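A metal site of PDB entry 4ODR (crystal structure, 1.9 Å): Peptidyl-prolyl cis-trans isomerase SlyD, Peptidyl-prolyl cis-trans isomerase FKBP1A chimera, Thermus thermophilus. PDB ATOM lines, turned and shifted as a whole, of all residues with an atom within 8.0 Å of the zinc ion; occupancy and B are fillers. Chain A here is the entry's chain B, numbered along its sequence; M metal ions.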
ATOM      1  N   THR A  91       0.246  -5.835 -22.601  1.00  0.00           N
ATOM      2  CA  THR A  91       0.844  -6.369 -21.390  1.00  0.00           C
ATOM      3  C   THR A  91      -0.240  -7.085 -20.586  1.00  0.00           C
ATOM      4  O   THR A  91      -1.416  -6.870 -20.836  1.00  0.00           O
ATOM      5  CB  THR A  91       1.472  -5.262 -20.532  1.00  0.00           C
ATOM      6  OG1 THR A  91       0.428  -4.439 -20.016  1.00  0.00           O
ATOM      7  CG2 THR A  91       2.436  -4.410 -21.361  1.00  0.00           C
ATOM      8  N   GLU A  93      -1.285  -6.541 -17.598  1.00  0.00           N
ATOM      9  CA  GLU A  93      -2.159  -5.639 -16.863  1.00  0.00           C
ATOM     10  C   GLU A  93      -3.103  -4.901 -17.798  1.00  0.00           C
ATOM     11  O   GLU A  93      -4.231  -4.603 -17.420  1.00  0.00           O
ATOM     12  CB  GLU A  93      -1.339  -4.640 -16.010  1.00  0.00           C
ATOM     13  CG  GLU A  93      -0.543  -5.298 -14.899  1.00  0.00           C
ATOM     14  CD  GLU A  93      -1.411  -5.837 -13.777  1.00  0.00           C
ATOM     15  OE1 GLU A  93      -2.557  -5.359 -13.627  1.00  0.00           O
ATOM     16  OE2 GLU A  93      -0.955  -6.737 -13.038  1.00  0.00           O
ATOM     17  N   GLU A  94      -2.651  -4.613 -19.022  1.00  0.00           N
ATOM     18  CA  GLU A  94      -3.532  -4.021 -20.026  1.00  0.00           C
ATOM     19  C   GLU A  94      -4.678  -4.979 -20.360  1.00  0.00           C
ATOM     20  O   GLU A  94      -5.847  -4.562 -20.424  1.00  0.00           O
ATOM     21  CB  GLU A  94      -2.759  -3.659 -21.302  1.00  0.00           C
ATOM     22  CG  GLU A  94      -1.891  -2.411 -21.166  1.00  0.00           C
ATOM     23  CD  GLU A  94      -1.015  -2.157 -22.392  1.00  0.00           C
ATOM     24  OE1 GLU A  94      -0.453  -3.139 -22.937  1.00  0.00           O
ATOM     25  OE2 GLU A  94      -0.897  -0.985 -22.805  1.00  0.00           O
ATOM     26  N   LEU A  95      -4.353  -6.245 -20.558  1.00  0.00           N
ATOM     27  CA  LEU A  95      -5.374  -7.254 -20.851  1.00  0.00           C
ATOM     28  C   LEU A  95      -6.362  -7.389 -19.701  1.00  0.00           C
ATOM     29  O   LEU A  95      -7.567  -7.436 -19.921  1.00  0.00           O
ATOM     30  CB  LEU A  95      -4.725  -8.617 -21.135  1.00  0.00           C
ATOM     31  CG  LEU A  95      -4.054  -8.776 -22.502  1.00  0.00           C
ATOM     32  CD1 LEU A  95      -3.380 -10.132 -22.625  1.00  0.00           C
ATOM     33  CD2 LEU A  95      -5.091  -8.580 -23.611  1.00  0.00           C
ATOM     34  N   LEU A  96      -5.847  -7.451 -18.479  1.00  0.00           N
ATOM     35  CA  LEU A  96      -6.697  -7.527 -17.298  1.00  0.00           C
ATOM     36  C   LEU A  96      -7.641  -6.327 -17.197  1.00  0.00           C
ATOM     37  O   LEU A  96      -8.840  -6.482 -16.984  1.00  0.00           O
ATOM     38  CB  LEU A  96      -5.838  -7.615 -16.030  1.00  0.00           C
ATOM     39  CG  LEU A  96      -6.612  -7.632 -14.703  1.00  0.00           C
ATOM     40  CD1 LEU A  96      -7.501  -8.862 -14.617  1.00  0.00           C
ATOM     41  CD2 LEU A  96      -5.648  -7.594 -13.519  1.00  0.00           C
ATOM     42  N   HIS A  97      -7.093  -5.125 -17.350  1.00  0.00           N
ATOM     43  CA  HIS A  97      -7.888  -3.911 -17.200  1.00  0.00           C
ATOM     44  C   HIS A  97      -8.790  -3.675 -18.404  1.00  0.00           C
ATOM     45  O   HIS A  97      -9.770  -2.921 -18.310  1.00  0.00           O
ATOM     46  CB  HIS A  97      -6.984  -2.703 -16.997  1.00  0.00           C
ATOM     47  CG  HIS A  97      -6.165  -2.762 -15.744  1.00  0.00           C
ATOM     48  ND1 HIS A  97      -5.205  -1.820 -15.440  1.00  0.00           N
ATOM     49  CD2 HIS A  97      -6.165  -3.657 -14.733  1.00  0.00           C
ATOM     50  CE1 HIS A  97      -4.654  -2.135 -14.287  1.00  0.00           C
ATOM     51  NE2 HIS A  97      -5.219  -3.237 -13.827  1.00  0.00           N
ATOM     52  N   GLY A  98      -8.449  -4.285 -19.527  1.00  0.00           N
ATOM     53  CA  GLY A  98      -9.223  -4.100 -20.747  1.00  0.00           C
ATOM     54  C   GLY A  98      -8.983  -2.757 -21.416  1.00  0.00           C
ATOM     55  O   GLY A  98      -9.844  -2.258 -22.144  1.00  0.00           O
ATOM     56  N   HIS A  99      -7.817  -2.170 -21.183  1.00  0.00           N
ATOM     57  CA  HIS A  99      -7.485  -0.903 -21.825  1.00  0.00           C
ATOM     58  C   HIS A  99      -5.985  -0.739 -22.044  1.00  0.00           C
ATOM     59  O   HIS A  99      -5.191  -1.507 -21.490  1.00  0.00           O
ATOM     60  CB  HIS A  99      -8.041   0.288 -21.018  1.00  0.00           C
ATOM     61  CG  HIS A  99      -7.517   0.406 -19.612  1.00  0.00           C
ATOM     62  ND1 HIS A  99      -8.264   0.975 -18.602  1.00  0.00           N
ATOM     63  CD2 HIS A  99      -6.334   0.058 -19.041  1.00  0.00           C
ATOM     64  CE1 HIS A  99      -7.572   0.967 -17.469  1.00  0.00           C
ATOM     65  NE2 HIS A  99      -6.393   0.422 -17.720  1.00  0.00           N
ATOM     66  N   ALA A 100      -5.606   0.257 -22.829  1.00  0.00           N
ATOM     67  CA  ALA A 100      -4.194   0.550 -23.112  1.00  0.00           C
ATOM     68  C   ALA A 100      -3.530   1.355 -21.985  1.00  0.00           C
ATOM     69  O   ALA A 100      -4.172   2.163 -21.327  1.00  0.00           O
ATOM     70  CB  ALA A 100      -4.064   1.294 -24.432  1.00  0.00           C
ATOM     71  N   HIS A 101      -2.249   1.101 -21.786  1.00  0.00           N
ATOM     72  CA  HIS A 101      -1.416   1.834 -20.833  1.00  0.00           C
ATOM     73  C   HIS A 101      -0.361   2.612 -21.602  1.00  0.00           C
ATOM     74  O   HIS A 101      -0.025   2.230 -22.708  1.00  0.00           O
ATOM     75  CB  HIS A 101      -0.731   0.873 -19.846  1.00  0.00           C
ATOM     76  CG  HIS A 101      -1.640   0.285 -18.816  1.00  0.00           C
ATOM     77  ND1 HIS A 101      -1.256  -0.755 -17.994  1.00  0.00           N
ATOM     78  CD2 HIS A 101      -2.912   0.595 -18.456  1.00  0.00           C
ATOM     79  CE1 HIS A 101      -2.237  -1.062 -17.182  1.00  0.00           C
ATOM     80  NE2 HIS A 101      -3.260  -0.247 -17.423  1.00  0.00           N
ATOM     81  N   PRO A 102       0.195   3.682 -21.005  1.00  0.00           N
ATOM     82  CA  PRO A 102       1.361   4.326 -21.601  1.00  0.00           C
ATOM     83  C   PRO A 102       2.539   3.367 -21.723  1.00  0.00           C
ATOM     84  O   PRO A 102       2.674   2.465 -20.897  1.00  0.00           O
ATOM     85  CB  PRO A 102       1.696   5.454 -20.619  1.00  0.00           C
ATOM     86  CG  PRO A 102       0.426   5.698 -19.855  1.00  0.00           C
ATOM     87  CD  PRO A 102      -0.234   4.355 -19.756  1.00  0.00           C
HETATM   88 ZN    ZN M   1      -4.941  -0.032 -16.392  1.00  0.00          ZN
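The side-chain carboxylate (OE2) of Glu 94 sits at hydrogen-bond distance from the backbone NH (N) of His 101 (2.7 Å). N of His 99 is in hydrogen-bond range of O of Glu 94 (3.2 Å). NE2 of His 97 lies within hydrogen-bond range of OE1 of Glu 93 (3.4 Å).
The zinc ion is bound by NE2 of His 101, NE2 of His 99 and ND1 of His 97.
Within 4 Å of the zinc ion: His 97, His 99 and His 101. The nearest printed residue that does not touch the zinc ion is Glu 93 (4.7 Å).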
